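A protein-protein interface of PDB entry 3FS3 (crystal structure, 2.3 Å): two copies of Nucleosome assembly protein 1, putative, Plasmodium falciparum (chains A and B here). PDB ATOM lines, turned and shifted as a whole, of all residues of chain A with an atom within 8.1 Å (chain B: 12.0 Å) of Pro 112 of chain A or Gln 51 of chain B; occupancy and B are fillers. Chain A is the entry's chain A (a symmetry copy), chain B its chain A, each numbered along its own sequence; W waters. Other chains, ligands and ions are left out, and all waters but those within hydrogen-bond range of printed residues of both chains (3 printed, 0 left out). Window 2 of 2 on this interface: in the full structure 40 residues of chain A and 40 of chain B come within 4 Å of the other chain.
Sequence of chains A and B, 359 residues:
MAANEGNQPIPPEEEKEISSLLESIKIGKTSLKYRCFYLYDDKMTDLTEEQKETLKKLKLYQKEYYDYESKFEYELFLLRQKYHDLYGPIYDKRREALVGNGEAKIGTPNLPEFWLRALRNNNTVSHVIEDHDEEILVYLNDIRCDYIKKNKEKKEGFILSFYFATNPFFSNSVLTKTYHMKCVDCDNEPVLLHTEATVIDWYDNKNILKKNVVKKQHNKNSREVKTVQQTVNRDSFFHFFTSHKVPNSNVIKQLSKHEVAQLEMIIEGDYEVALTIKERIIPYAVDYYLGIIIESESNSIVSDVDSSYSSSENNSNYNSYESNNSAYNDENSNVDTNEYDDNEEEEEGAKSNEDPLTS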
ATOM      1  N   ALA A  97     -18.392   0.246 -12.407  1.00  0.00           N
ATOM      2  CA  ALA A  97     -17.914   1.259 -13.333  1.00  0.00           C
ATOM      3  C   ALA A  97     -18.995   1.604 -14.358  1.00  0.00           C
ATOM      4  O   ALA A  97     -19.118   2.754 -14.768  1.00  0.00           O
ATOM      5  CB  ALA A  97     -16.657   0.764 -14.044  1.00  0.00           C
ATOM      6  N   LEU A  98     -19.776   0.607 -14.766  1.00  0.00           N
ATOM      7  CA  LEU A  98     -20.840   0.818 -15.751  1.00  0.00           C
ATOM      8  C   LEU A  98     -22.045   1.567 -15.192  1.00  0.00           C
ATOM      9  O   LEU A  98     -22.554   2.503 -15.816  1.00  0.00           O
ATOM     10  CB  LEU A  98     -21.334  -0.524 -16.309  1.00  0.00           C
ATOM     11  CG  LEU A  98     -20.478  -1.290 -17.317  1.00  0.00           C
ATOM     12  CD1 LEU A  98     -21.108  -2.650 -17.588  1.00  0.00           C
ATOM     13  CD2 LEU A  98     -20.379  -0.507 -18.612  1.00  0.00           C
ATOM     14  N   ILE A 106     -31.532   4.832 -16.850  1.00  0.00           N
ATOM     15  CA  ILE A 106     -30.990   4.285 -18.086  1.00  0.00           C
ATOM     16  C   ILE A 106     -29.966   3.203 -17.767  1.00  0.00           C
ATOM     17  O   ILE A 106     -29.301   3.250 -16.733  1.00  0.00           O
ATOM     18  CB  ILE A 106     -30.363   5.395 -18.974  1.00  0.00           C
ATOM     19  CG1 ILE A 106     -30.134   4.852 -20.385  1.00  0.00           C
ATOM     20  CG2 ILE A 106     -29.072   5.905 -18.373  1.00  0.00           C
ATOM     21  CD1 ILE A 106     -31.432   4.460 -21.119  1.00  0.00           C
ATOM     22  N   GLY A 107     -29.865   2.210 -18.644  1.00  0.00           N
ATOM     23  CA  GLY A 107     -28.932   1.119 -18.417  1.00  0.00           C
ATOM     24  C   GLY A 107     -27.495   1.567 -18.550  1.00  0.00           C
ATOM     25  O   GLY A 107     -27.198   2.384 -19.409  1.00  0.00           O
ATOM     26  N   THR A 108     -26.614   1.053 -17.696  1.00  0.00           N
ATOM     27  CA  THR A 108     -25.189   1.390 -17.743  1.00  0.00           C
ATOM     28  C   THR A 108     -24.951   2.836 -18.200  1.00  0.00           C
ATOM     29  O   THR A 108     -24.360   3.072 -19.248  1.00  0.00           O
ATOM     30  CB  THR A 108     -24.445   0.425 -18.702  1.00  0.00           C
ATOM     31  OG1 THR A 108     -24.947   0.587 -20.036  1.00  0.00           O
ATOM     32  CG2 THR A 108     -24.663  -1.025 -18.277  1.00  0.00           C
ATOM     33  N   PRO A 109     -25.399   3.824 -17.407  1.00  0.00           N
ATOM     34  CA  PRO A 109     -25.220   5.232 -17.774  1.00  0.00           C
ATOM     35  C   PRO A 109     -23.795   5.706 -18.027  1.00  0.00           C
ATOM     36  O   PRO A 109     -23.595   6.671 -18.763  1.00  0.00           O
ATOM     37  CB  PRO A 109     -25.896   5.981 -16.624  1.00  0.00           C
ATOM     38  CG  PRO A 109     -25.681   5.059 -15.455  1.00  0.00           C
ATOM     39  CD  PRO A 109     -25.964   3.700 -16.050  1.00  0.00           C
ATOM     40  N   ASN A 110     -22.798   5.052 -17.444  1.00  0.00           N
ATOM     41  CA  ASN A 110     -21.430   5.500 -17.685  1.00  0.00           C
ATOM     42  C   ASN A 110     -20.879   4.986 -19.012  1.00  0.00           C
ATOM     43  O   ASN A 110     -19.772   5.347 -19.410  1.00  0.00           O
ATOM     44  CB  ASN A 110     -20.518   5.101 -16.527  1.00  0.00           C
ATOM     45  CG  ASN A 110     -20.998   5.661 -15.199  1.00  0.00           C
ATOM     46  OD1 ASN A 110     -21.375   6.829 -15.105  1.00  0.00           O
ATOM     47  ND2 ASN A 110     -20.979   4.833 -14.163  1.00  0.00           N
ATOM     48  N   LEU A 111     -21.654   4.139 -19.691  1.00  0.00           N
ATOM     49  CA  LEU A 111     -21.278   3.602 -21.004  1.00  0.00           C
ATOM     50  C   LEU A 111     -22.552   3.083 -21.672  1.00  0.00           C
ATOM     51  O   LEU A 111     -22.837   1.875 -21.686  1.00  0.00           O
ATOM     52  CB  LEU A 111     -20.245   2.478 -20.881  1.00  0.00           C
ATOM     53  CG  LEU A 111     -19.564   2.101 -22.200  1.00  0.00           C
ATOM     54  CD1 LEU A 111     -18.872   3.332 -22.777  1.00  0.00           C
ATOM     55  CD2 LEU A 111     -18.547   0.987 -21.975  1.00  0.00           C
ATOM     56  N   PRO A 112     -23.340   4.012 -22.236  1.00  0.00           N
ATOM     57  CA  PRO A 112     -24.609   3.782 -22.924  1.00  0.00           C
ATOM     58  C   PRO A 112     -24.680   2.568 -23.837  1.00  0.00           C
ATOM     59  O   PRO A 112     -23.804   2.358 -24.672  1.00  0.00           O
ATOM     60  CB  PRO A 112     -24.826   5.095 -23.682  1.00  0.00           C
ATOM     61  CG  PRO A 112     -24.269   6.100 -22.749  1.00  0.00           C
ATOM     62  CD  PRO A 112     -22.960   5.435 -22.327  1.00  0.00           C
ATOM     63  N   GLU A 113     -25.739   1.776 -23.665  1.00  0.00           N
ATOM     64  CA  GLU A 113     -25.991   0.593 -24.490  1.00  0.00           C
ATOM     65  C   GLU A 113     -24.949  -0.514 -24.421  1.00  0.00           C
ATOM     66  O   GLU A 113     -24.899  -1.377 -25.306  1.00  0.00           O
ATOM     67  CB  GLU A 113     -26.174   1.013 -25.957  1.00  0.00           C
ATOM     68  CG  GLU A 113     -26.933   2.310 -26.116  1.00  0.00           C
ATOM     69  CD  GLU A 113     -27.402   2.559 -27.538  1.00  0.00           C
ATOM     70  OE1 GLU A 113     -26.745   2.077 -28.491  1.00  0.00           O
ATOM     71  OE2 GLU A 113     -28.427   3.255 -27.700  1.00  0.00           O
ATOM     72  N   PHE A 114     -24.140  -0.513 -23.363  1.00  0.00           N
ATOM     73  CA  PHE A 114     -23.097  -1.520 -23.216  1.00  0.00           C
ATOM     74  C   PHE A 114     -23.509  -2.962 -23.476  1.00  0.00           C
ATOM     75  O   PHE A 114     -22.910  -3.635 -24.305  1.00  0.00           O
ATOM     76  CB  PHE A 114     -22.469  -1.468 -21.822  1.00  0.00           C
ATOM     77  CG  PHE A 114     -21.414  -2.522 -21.611  1.00  0.00           C
ATOM     78  CD1 PHE A 114     -20.149  -2.382 -22.186  1.00  0.00           C
ATOM     79  CD2 PHE A 114     -21.704  -3.674 -20.894  1.00  0.00           C
ATOM     80  CE1 PHE A 114     -19.186  -3.383 -22.048  1.00  0.00           C
ATOM     81  CE2 PHE A 114     -20.755  -4.682 -20.745  1.00  0.00           C
ATOM     82  CZ  PHE A 114     -19.483  -4.534 -21.328  1.00  0.00           C
ATOM     83  N   TRP A 115     -24.509  -3.450 -22.752  1.00  0.00           N
ATOM     84  CA  TRP A 115     -24.925  -4.838 -22.921  1.00  0.00           C
ATOM     85  C   TRP A 115     -25.622  -5.100 -24.254  1.00  0.00           C
ATOM     86  O   TRP A 115     -25.405  -6.144 -24.873  1.00  0.00           O
ATOM     87  CB  TRP A 115     -25.814  -5.287 -21.752  1.00  0.00           C
ATOM     88  CG  TRP A 115     -25.104  -5.261 -20.444  1.00  0.00           C
ATOM     89  CD1 TRP A 115     -25.226  -4.316 -19.465  1.00  0.00           C
ATOM     90  CD2 TRP A 115     -24.115  -6.191 -19.984  1.00  0.00           C
ATOM     91  NE1 TRP A 115     -24.372  -4.599 -18.426  1.00  0.00           N
ATOM     92  CE2 TRP A 115     -23.677  -5.741 -18.718  1.00  0.00           C
ATOM     93  CE3 TRP A 115     -23.556  -7.360 -20.519  1.00  0.00           C
ATOM     94  CZ2 TRP A 115     -22.707  -6.420 -17.973  1.00  0.00           C
ATOM     95  CZ3 TRP A 115     -22.593  -8.036 -19.781  1.00  0.00           C
ATOM     96  CH2 TRP A 115     -22.178  -7.562 -18.517  1.00  0.00           C
ATOM     97  N   LEU A 116     -26.452  -4.163 -24.702  1.00  0.00           N
ATOM     98  CA  LEU A 116     -27.123  -4.355 -25.978  1.00  0.00           C
ATOM     99  C   LEU A 116     -26.081  -4.583 -27.057  1.00  0.00           C
ATOM    100  O   LEU A 116     -26.202  -5.517 -27.850  1.00  0.00           O
ATOM    101  CB  LEU A 116     -27.970  -3.146 -26.362  1.00  0.00           C
ATOM    102  CG  LEU A 116     -28.455  -3.201 -27.823  1.00  0.00           C
ATOM    103  CD1 LEU A 116     -29.240  -4.492 -28.058  1.00  0.00           C
ATOM    104  CD2 LEU A 116     -29.320  -1.983 -28.145  1.00  0.00           C
ATOM    105  N   ARG A 117     -25.053  -3.739 -27.083  1.00  0.00           N
ATOM    106  CA  ARG A 117     -24.021  -3.867 -28.102  1.00  0.00           C
ATOM    107  C   ARG A 117     -23.189  -5.126 -27.948  1.00  0.00           C
ATOM    108  O   ARG A 117     -22.840  -5.762 -28.937  1.00  0.00           O
ATOM    109  CB  ARG A 117     -23.140  -2.622 -28.124  1.00  0.00           C
ATOM    110  CG  ARG A 117     -23.893  -1.424 -28.669  1.00  0.00           C
ATOM    111  CD  ARG A 117     -23.041  -0.179 -28.799  1.00  0.00           C
ATOM    112  NE  ARG A 117     -23.865   0.974 -29.157  1.00  0.00           N
ATOM    113  CZ  ARG A 117     -23.456   2.239 -29.105  1.00  0.00           C
ATOM    114  NH1 ARG A 117     -22.222   2.527 -28.707  1.00  0.00           N
ATOM    115  NH2 ARG A 117     -24.287   3.217 -29.443  1.00  0.00           N
ATOM    116  N   LEU A 137     -33.571  -3.265 -24.191  1.00  0.00           N
ATOM    117  CA  LEU A 137     -32.246  -3.707 -23.784  1.00  0.00           C
ATOM    118  C   LEU A 137     -31.277  -2.582 -23.393  1.00  0.00           C
ATOM    119  O   LEU A 137     -30.292  -2.820 -22.693  1.00  0.00           O
ATOM    120  CB  LEU A 137     -31.647  -4.594 -24.887  1.00  0.00           C
ATOM    121  CG  LEU A 137     -32.372  -5.929 -25.112  1.00  0.00           C
ATOM    122  CD1 LEU A 137     -31.850  -6.588 -26.389  1.00  0.00           C
ATOM    123  CD2 LEU A 137     -32.164  -6.856 -23.891  1.00  0.00           C
ATOM    124  N   VAL A 138     -31.553  -1.360 -23.834  1.00  0.00           N
ATOM    125  CA  VAL A 138     -30.702  -0.233 -23.485  1.00  0.00           C
ATOM    126  C   VAL A 138     -30.820   0.085 -21.987  1.00  0.00           C
ATOM    127  O   VAL A 138     -30.012   0.833 -21.444  1.00  0.00           O
ATOM    128  CB  VAL A 138     -31.066   1.040 -24.294  1.00  0.00           C
ATOM    129  CG1 VAL A 138     -30.827   0.800 -25.793  1.00  0.00           C
ATOM    130  CG2 VAL A 138     -32.514   1.434 -24.031  1.00  0.00           C
ATOM    131  N   LEU A 140     -30.647  -2.260 -19.776  1.00  0.00           N
ATOM    132  CA  LEU A 140     -29.921  -3.338 -19.119  1.00  0.00           C
ATOM    133  C   LEU A 140     -28.715  -2.779 -18.337  1.00  0.00           C
ATOM    134  O   LEU A 140     -27.891  -2.047 -18.892  1.00  0.00           O
ATOM    135  CB  LEU A 140     -29.496  -4.361 -20.191  1.00  0.00           C
ATOM    136  CG  LEU A 140     -29.360  -5.844 -19.826  1.00  0.00           C
ATOM    137  CD1 LEU A 140     -30.515  -6.283 -18.938  1.00  0.00           C
ATOM    138  CD2 LEU A 140     -29.311  -6.682 -21.099  1.00  0.00           C
ATOM    139  N   TYR A 289     -18.555  -5.990 -26.812  1.00  0.00           N
ATOM    140  CA  TYR A 289     -18.959  -4.604 -27.013  1.00  0.00           C
ATOM    141  C   TYR A 289     -18.067  -3.994 -28.097  1.00  0.00           C
ATOM    142  O   TYR A 289     -18.568  -3.430 -29.066  1.00  0.00           O
ATOM    143  CB  TYR A 289     -18.809  -3.815 -25.715  1.00  0.00           C
ATOM    144  CG  TYR A 289     -18.944  -2.322 -25.886  1.00  0.00           C
ATOM    145  CD1 TYR A 289     -20.184  -1.692 -25.781  1.00  0.00           C
ATOM    146  CD2 TYR A 289     -17.826  -1.534 -26.154  1.00  0.00           C
ATOM    147  CE1 TYR A 289     -20.304  -0.303 -25.940  1.00  0.00           C
ATOM    148  CE2 TYR A 289     -17.933  -0.155 -26.315  1.00  0.00           C
ATOM    149  CZ  TYR A 289     -19.170   0.456 -26.204  1.00  0.00           C
ATOM    150  OH  TYR A 289     -19.257   1.828 -26.342  1.00  0.00           O
ATOM    151  N   THR B  45     -14.059   5.193 -28.596  1.00  0.00           N
ATOM    152  CA  THR B  45     -14.208   5.699 -29.988  1.00  0.00           C
ATOM    153  C   THR B  45     -14.865   7.085 -30.036  1.00  0.00           C
ATOM    154  O   THR B  45     -14.191   8.098 -29.864  1.00  0.00           O
ATOM    155  CB  THR B  45     -15.010   4.698 -30.866  1.00  0.00           C
ATOM    156  OG1 THR B  45     -15.712   3.772 -30.031  1.00  0.00           O
ATOM    157  CG2 THR B  45     -14.073   3.918 -31.784  1.00  0.00           C
ATOM    158  N   ASP B  46     -16.172   7.139 -30.263  1.00  0.00           N
ATOM    159  CA  ASP B  46     -16.862   8.426 -30.318  1.00  0.00           C
ATOM    160  C   ASP B  46     -17.713   8.655 -29.075  1.00  0.00           C
ATOM    161  O   ASP B  46     -18.827   9.185 -29.124  1.00  0.00           O
ATOM    162  CB  ASP B  46     -17.697   8.510 -31.588  1.00  0.00           C
ATOM    163  CG  ASP B  46     -16.842   8.398 -32.836  1.00  0.00           C
ATOM    164  OD1 ASP B  46     -15.832   9.131 -32.919  1.00  0.00           O
ATOM    165  OD2 ASP B  46     -17.173   7.582 -33.724  1.00  0.00           O
ATOM    166  N   LEU B  47     -17.139   8.245 -27.954  1.00  0.00           N
ATOM    167  CA  LEU B  47     -17.758   8.370 -26.654  1.00  0.00           C
ATOM    168  C   LEU B  47     -17.270   9.687 -26.061  1.00  0.00           C
ATOM    169  O   LEU B  47     -16.329  10.293 -26.571  1.00  0.00           O
ATOM    170  CB  LEU B  47     -17.284   7.219 -25.771  1.00  0.00           C
ATOM    171  CG  LEU B  47     -17.216   5.862 -26.468  1.00  0.00           C
ATOM    172  CD1 LEU B  47     -16.318   4.900 -25.699  1.00  0.00           C
ATOM    173  CD2 LEU B  47     -18.618   5.317 -26.605  1.00  0.00           C
ATOM    174  N   THR B  48     -17.916  10.136 -24.994  1.00  0.00           N
ATOM    175  CA  THR B  48     -17.486  11.357 -24.327  1.00  0.00           C
ATOM    176  C   THR B  48     -16.201  10.935 -23.619  1.00  0.00           C
ATOM    177  O   THR B  48     -15.963   9.732 -23.434  1.00  0.00           O
ATOM    178  CB  THR B  48     -18.500  11.801 -23.272  1.00  0.00           C
ATOM    179  OG1 THR B  48     -18.789  10.694 -22.408  1.00  0.00           O
ATOM    180  CG2 THR B  48     -19.787  12.292 -23.929  1.00  0.00           C
ATOM    181  N   GLU B  49     -15.374  11.900 -23.225  1.00  0.00           N
ATOM    182  CA  GLU B  49     -14.126  11.573 -22.546  1.00  0.00           C
ATOM    183  C   GLU B  49     -14.401  10.715 -21.314  1.00  0.00           C
ATOM    184  O   GLU B  49     -13.660   9.780 -21.000  1.00  0.00           O
ATOM    185  CB  GLU B  49     -13.386  12.853 -22.145  1.00  0.00           C
ATOM    186  CG  GLU B  49     -12.817  13.607 -23.329  1.00  0.00           C
ATOM    187  CD  GLU B  49     -12.002  12.710 -24.251  1.00  0.00           C
ATOM    188  OE1 GLU B  49     -11.099  11.998 -23.762  1.00  0.00           O
ATOM    189  OE2 GLU B  49     -12.269  12.717 -25.468  1.00  0.00           O
ATOM    190  N   GLU B  50     -15.486  11.045 -20.629  1.00  0.00           N
ATOM    191  CA  GLU B  50     -15.915  10.333 -19.433  1.00  0.00           C
ATOM    192  C   GLU B  50     -16.174   8.851 -19.731  1.00  0.00           C
ATOM    193  O   GLU B  50     -15.751   7.967 -18.985  1.00  0.00           O
ATOM    194  CB  GLU B  50     -17.189  11.000 -18.914  1.00  0.00           C
ATOM    195  CG  GLU B  50     -17.902  10.278 -17.803  1.00  0.00           C
ATOM    196  CD  GLU B  50     -19.339  10.745 -17.673  1.00  0.00           C
ATOM    197  OE1 GLU B  50     -20.016  10.326 -16.712  1.00  0.00           O
ATOM    198  OE2 GLU B  50     -19.792  11.525 -18.542  1.00  0.00           O
ATOM    199  N   GLN B  51     -16.875   8.581 -20.825  1.00  0.00           N
ATOM    200  CA  GLN B  51     -17.179   7.206 -21.199  1.00  0.00           C
ATOM    201  C   GLN B  51     -15.913   6.482 -21.657  1.00  0.00           C
ATOM    202  O   GLN B  51     -15.761   5.276 -21.432  1.00  0.00           O
ATOM    203  CB  GLN B  51     -18.251   7.197 -22.293  1.00  0.00           C
ATOM    204  CG  GLN B  51     -19.561   7.861 -21.844  1.00  0.00           C
ATOM    205  CD  GLN B  51     -20.478   8.225 -23.003  1.00  0.00           C
ATOM    206  OE1 GLN B  51     -20.082   8.176 -24.167  1.00  0.00           O
ATOM    207  NE2 GLN B  51     -21.705   8.611 -22.683  1.00  0.00           N
ATOM    208  N   LYS B  52     -14.996   7.217 -22.285  1.00  0.00           N
ATOM    209  CA  LYS B  52     -13.751   6.613 -22.752  1.00  0.00           C
ATOM    210  C   LYS B  52     -13.010   6.042 -21.548  1.00  0.00           C
ATOM    211  O   LYS B  52     -12.461   4.948 -21.619  1.00  0.00           O
ATOM    212  CB  LYS B  52     -12.868   7.646 -23.461  1.00  0.00           C
ATOM    213  CG  LYS B  52     -13.425   8.172 -24.773  1.00  0.00           C
ATOM    214  CD  LYS B  52     -12.516   9.261 -25.329  1.00  0.00           C
ATOM    215  CE  LYS B  52     -13.111   9.931 -26.556  1.00  0.00           C
ATOM    216  NZ  LYS B  52     -13.089   9.021 -27.728  1.00  0.00           N
ATOM    217  N   GLU B  53     -13.004   6.787 -20.446  1.00  0.00           N
ATOM    218  CA  GLU B  53     -12.344   6.341 -19.219  1.00  0.00           C
ATOM    219  C   GLU B  53     -12.981   5.055 -18.706  1.00  0.00           C
ATOM    220  O   GLU B  53     -12.289   4.125 -18.286  1.00  0.00           O
ATOM    221  CB  GLU B  53     -12.439   7.416 -18.133  1.00  0.00           C
ATOM    222  CG  GLU B  53     -11.337   8.442 -18.194  1.00  0.00           C
ATOM    223  CD  GLU B  53      -9.974   7.811 -18.005  1.00  0.00           C
ATOM    224  OE1 GLU B  53      -9.755   7.202 -16.935  1.00  0.00           O
ATOM    225  OE2 GLU B  53      -9.130   7.916 -18.924  1.00  0.00           O
ATOM    226  N   THR B  54     -14.309   5.020 -18.741  1.00  0.00           N
ATOM    227  CA  THR B  54     -15.066   3.860 -18.298  1.00  0.00           C
ATOM    228  C   THR B  54     -14.690   2.638 -19.134  1.00  0.00           C
ATOM    229  O   THR B  54     -14.524   1.538 -18.606  1.00  0.00           O
ATOM    230  CB  THR B  54     -16.573   4.119 -18.426  1.00  0.00           C
ATOM    231  OG1 THR B  54     -16.963   5.100 -17.458  1.00  0.00           O
ATOM    232  CG2 THR B  54     -17.363   2.828 -18.211  1.00  0.00           C
ATOM    233  N   LEU B  55     -14.549   2.847 -20.440  1.00  0.00           N
ATOM    234  CA  LEU B  55     -14.190   1.772 -21.350  1.00  0.00           C
ATOM    235  C   LEU B  55     -12.784   1.250 -21.043  1.00  0.00           C
ATOM    236  O   LEU B  55     -12.545   0.042 -21.077  1.00  0.00           O
ATOM    237  CB  LEU B  55     -14.265   2.263 -22.799  1.00  0.00           C
ATOM    238  CG  LEU B  55     -14.044   1.187 -23.862  1.00  0.00           C
ATOM    239  CD1 LEU B  55     -15.113   0.121 -23.722  1.00  0.00           C
ATOM    240  CD2 LEU B  55     -14.108   1.808 -25.256  1.00  0.00           C
ATOM    241  N   LYS B  56     -11.860   2.159 -20.742  1.00  0.00           N
ATOM    242  CA  LYS B  56     -10.490   1.756 -20.429  1.00  0.00           C
ATOM    243  C   LYS B  56     -10.487   0.922 -19.156  1.00  0.00           C
ATOM    244  O   LYS B  56      -9.788  -0.080 -19.073  1.00  0.00           O
ATOM    245  CB  LYS B  56      -9.585   2.981 -20.245  1.00  0.00           C
ATOM    246  CG  LYS B  56      -9.669   3.984 -21.386  1.00  0.00           C
ATOM    247  CD  LYS B  56      -9.415   3.341 -22.742  1.00  0.00           C
ATOM    248  CE  LYS B  56     -10.046   4.168 -23.860  1.00  0.00           C
ATOM    249  NZ  LYS B  56      -9.642   5.600 -23.801  1.00  0.00           N
ATOM    250  N   LYS B  57     -11.272   1.333 -18.166  1.00  0.00           N
ATOM    251  CA  LYS B  57     -11.333   0.581 -16.923  1.00  0.00           C
ATOM    252  C   LYS B  57     -11.835  -0.838 -17.186  1.00  0.00           C
ATOM    253  O   LYS B  57     -11.277  -1.803 -16.657  1.00  0.00           O
ATOM    254  CB  LYS B  57     -12.229   1.296 -15.913  1.00  0.00           C
ATOM    255  CG  LYS B  57     -11.600   2.565 -15.340  1.00  0.00           C
ATOM    256  CD  LYS B  57     -12.601   3.384 -14.523  1.00  0.00           C
ATOM    257  CE  LYS B  57     -13.110   2.628 -13.303  1.00  0.00           C
ATOM    258  NZ  LYS B  57     -14.149   3.409 -12.566  1.00  0.00           N
ATOM    259  N   LEU B  58     -12.867  -0.962 -18.023  1.00  0.00           N
ATOM    260  CA  LEU B  58     -13.420  -2.270 -18.361  1.00  0.00           C
ATOM    261  C   LEU B  58     -12.376  -3.162 -19.044  1.00  0.00           C
ATOM    262  O   LEU B  58     -12.304  -4.360 -18.756  1.00  0.00           O
ATOM    263  CB  LEU B  58     -14.653  -2.125 -19.270  1.00  0.00           C
ATOM    264  CG  LEU B  58     -16.018  -2.032 -18.588  1.00  0.00           C
ATOM    265  CD1 LEU B  58     -15.973  -0.998 -17.482  1.00  0.00           C
ATOM    266  CD2 LEU B  58     -17.093  -1.690 -19.615  1.00  0.00           C
ATOM    267  N   LYS B  59     -11.580  -2.593 -19.950  1.00  0.00           N
ATOM    268  CA  LYS B  59     -10.551  -3.384 -20.619  1.00  0.00           C
ATOM    269  C   LYS B  59      -9.540  -3.839 -19.571  1.00  0.00           C
ATOM    270  O   LYS B  59      -9.039  -4.965 -19.616  1.00  0.00           O
ATOM    271  CB  LYS B  59      -9.845  -2.574 -21.708  1.00  0.00           C
ATOM    272  CG  LYS B  59     -10.700  -2.305 -22.952  1.00  0.00           C
ATOM    273  CD  LYS B  59     -11.473  -3.555 -23.406  1.00  0.00           C
ATOM    274  CE  LYS B  59     -10.578  -4.777 -23.629  1.00  0.00           C
ATOM    275  NZ  LYS B  59      -9.695  -4.649 -24.824  1.00  0.00           N
ATOM    276  N   LEU B  60      -9.259  -2.958 -18.615  1.00  0.00           N
ATOM    277  CA  LEU B  60      -8.335  -3.288 -17.542  1.00  0.00           C
ATOM    278  C   LEU B  60      -8.901  -4.503 -16.805  1.00  0.00           C
ATOM    279  O   LEU B  60      -8.205  -5.501 -16.633  1.00  0.00           O
ATOM    280  CB  LEU B  60      -8.189  -2.111 -16.576  1.00  0.00           C
ATOM    281  CG  LEU B  60      -7.116  -2.293 -15.506  1.00  0.00           C
ATOM    282  CD1 LEU B  60      -5.747  -2.306 -16.180  1.00  0.00           C
ATOM    283  CD2 LEU B  60      -7.196  -1.166 -14.479  1.00  0.00           C
ATOM    284  N   TYR B  61     -10.170  -4.429 -16.397  1.00  0.00           N
ATOM    285  CA  TYR B  61     -10.794  -5.544 -15.691  1.00  0.00           C
ATOM    286  C   TYR B  61     -10.827  -6.788 -16.571  1.00  0.00           C
ATOM    287  O   TYR B  61     -10.616  -7.897 -16.088  1.00  0.00           O
ATOM    288  CB  TYR B  61     -12.226  -5.209 -15.258  1.00  0.00           C
ATOM    289  CG  TYR B  61     -12.375  -3.921 -14.476  1.00  0.00           C
ATOM    290  CD1 TYR B  61     -11.407  -3.514 -13.555  1.00  0.00           C
ATOM    291  CD2 TYR B  61     -13.485  -3.100 -14.668  1.00  0.00           C
ATOM    292  CE1 TYR B  61     -11.540  -2.318 -12.857  1.00  0.00           C
ATOM    293  CE2 TYR B  61     -13.631  -1.908 -13.979  1.00  0.00           C
ATOM    294  CZ  TYR B  61     -12.653  -1.517 -13.079  1.00  0.00           C
ATOM    295  OH  TYR B  61     -12.779  -0.307 -12.438  1.00  0.00           O
HETATM  296  O   HOH W   1     -18.341   7.248 -18.047  1.00  0.00           O
HETATM  297  O   HOH W   2     -17.880   2.403 -28.559  1.00  0.00           O
HETATM  298  O   HOH W   3     -22.173   8.837 -19.749  1.00  0.00           O
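No residue of chain B comes within 4 Å of Gly 107 of chain A.
No residue of chain B comes within 4 Å of Thr 108 of chain A.
Leu 111 of chain A touches just these residues of chain B: Gln 51, Thr 54, Leu 55 and Leu 58.
No residue of chain B comes within 4 Å of Val 138 of chain A.
Printed residues of chain B within 4 Å of Tyr 289 of chain A: Leu 47 and Leu 55.
Of chain A, only Asn 110 (3.5 Å), Leu 111 (3.9 Å) and Pro 112 (3.4 Å) come within 4 Å of Gln 51 of chain B.
Of the printed residues of chain A, Thr 54 of chain B touches Ala 97, Asn 110 and Leu 111.
Printed residues of chain A within 4 Å of Lys 57 of chain B: Ala 97.
Printed residues of chain A within 4 Å of Leu 58 of chain B: Ala 97, Leu 98, Leu 111 and Phe 114.
Leu 60 of chain B touches none of the printed residues of chain A.
The nearest residue of chain B that does not touch Pro 112 of chain A is Leu 47 of chain B (6.1 Å).
Of the 18 printed residues of chain A, 7 touch a printed residue of chain B.
Hydrophobic or aromatic side chains of chain A that line the printed part of chain B: Ala 97, Leu 98, Leu 111, Pro 112, Phe 114 and Tyr 289.
Hydrophobic or aromatic side chains of chain B that line the printed part of chain A: Leu 47, Leu 55 and Leu 58.
Among the printed residues, 14 pairs touch across the chains.
Among the printed residues, no Asp or Glu carboxylate lies within 4 Å of a Lys or Arg side-chain nitrogen of the other chain.
No position is printed for both chains.
Of the 14 pairs that touch across the chains among the printed residues, none has its exchanged pair printed and touching as well.
Water W1 lies within hydrogen-bond range of OG1 of Thr 54 of chain B, O of Asn 110 of chain A, O of Glu 50 of chain B and N of Gln 51 of chain B.
Water W3 lies within hydrogen-bond range of the backbone carbonyl oxygen of Pro 109 of chain A (2.8 Å) and the side-chain amide nitrogen of Gln 51 of chain B (3.0 Å).
OE1 of Gln 51 of chain B sits at hydrogen-bond distance from N of Thr 48 of chain B, at 3.0 Å.
O of Glu 50 of chain B sits at hydrogen-bond distance from OG1 of Thr 54 of chain B.
O of Ala 97 of chain A sits at hydrogen-bond distance from ND2 of Asn 110 of chain A, 2.9 Å away.
Among the printed residues, pairs that only touch across the chains: Ala 97 of chain A with Thr 54 of chain B (3.9 Å), Ala 97 of chain A with Lys 57 of chain B (3.9 Å), Ala 97 of chain A with Leu 58 of chain B (3.9 Å), Leu 98 of chain A with Leu 58 of chain B (3.6 Å), Asn 110 of chain A with Gln 51 of chain B (3.5 Å), Leu 111 of chain A with Gln 51 of chain B (3.9 Å), Leu 111 of chain A with Thr 54 of chain B (3.9 Å), Leu 111 of chain A with Leu 55 of chain B (3.9 Å), Leu 111 of chain A with Leu 58 of chain B (3.9 Å), Pro 112 of chain A with Gln 51 of chain B (3.4 Å), Phe 114 of chain A with Leu 58 of chain B (3.6 Å), Tyr 289 of chain A with Leu 47 of chain B (3.6 Å) and Tyr 289 of chain A with Leu 55 of chain B (3.8 Å).
The backbone carbonyl oxygen of Asn 110 of chain A is in hydrogen-bond range of the side-chain hydroxyl of Thr 54 of chain B, 3.4 Å away.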
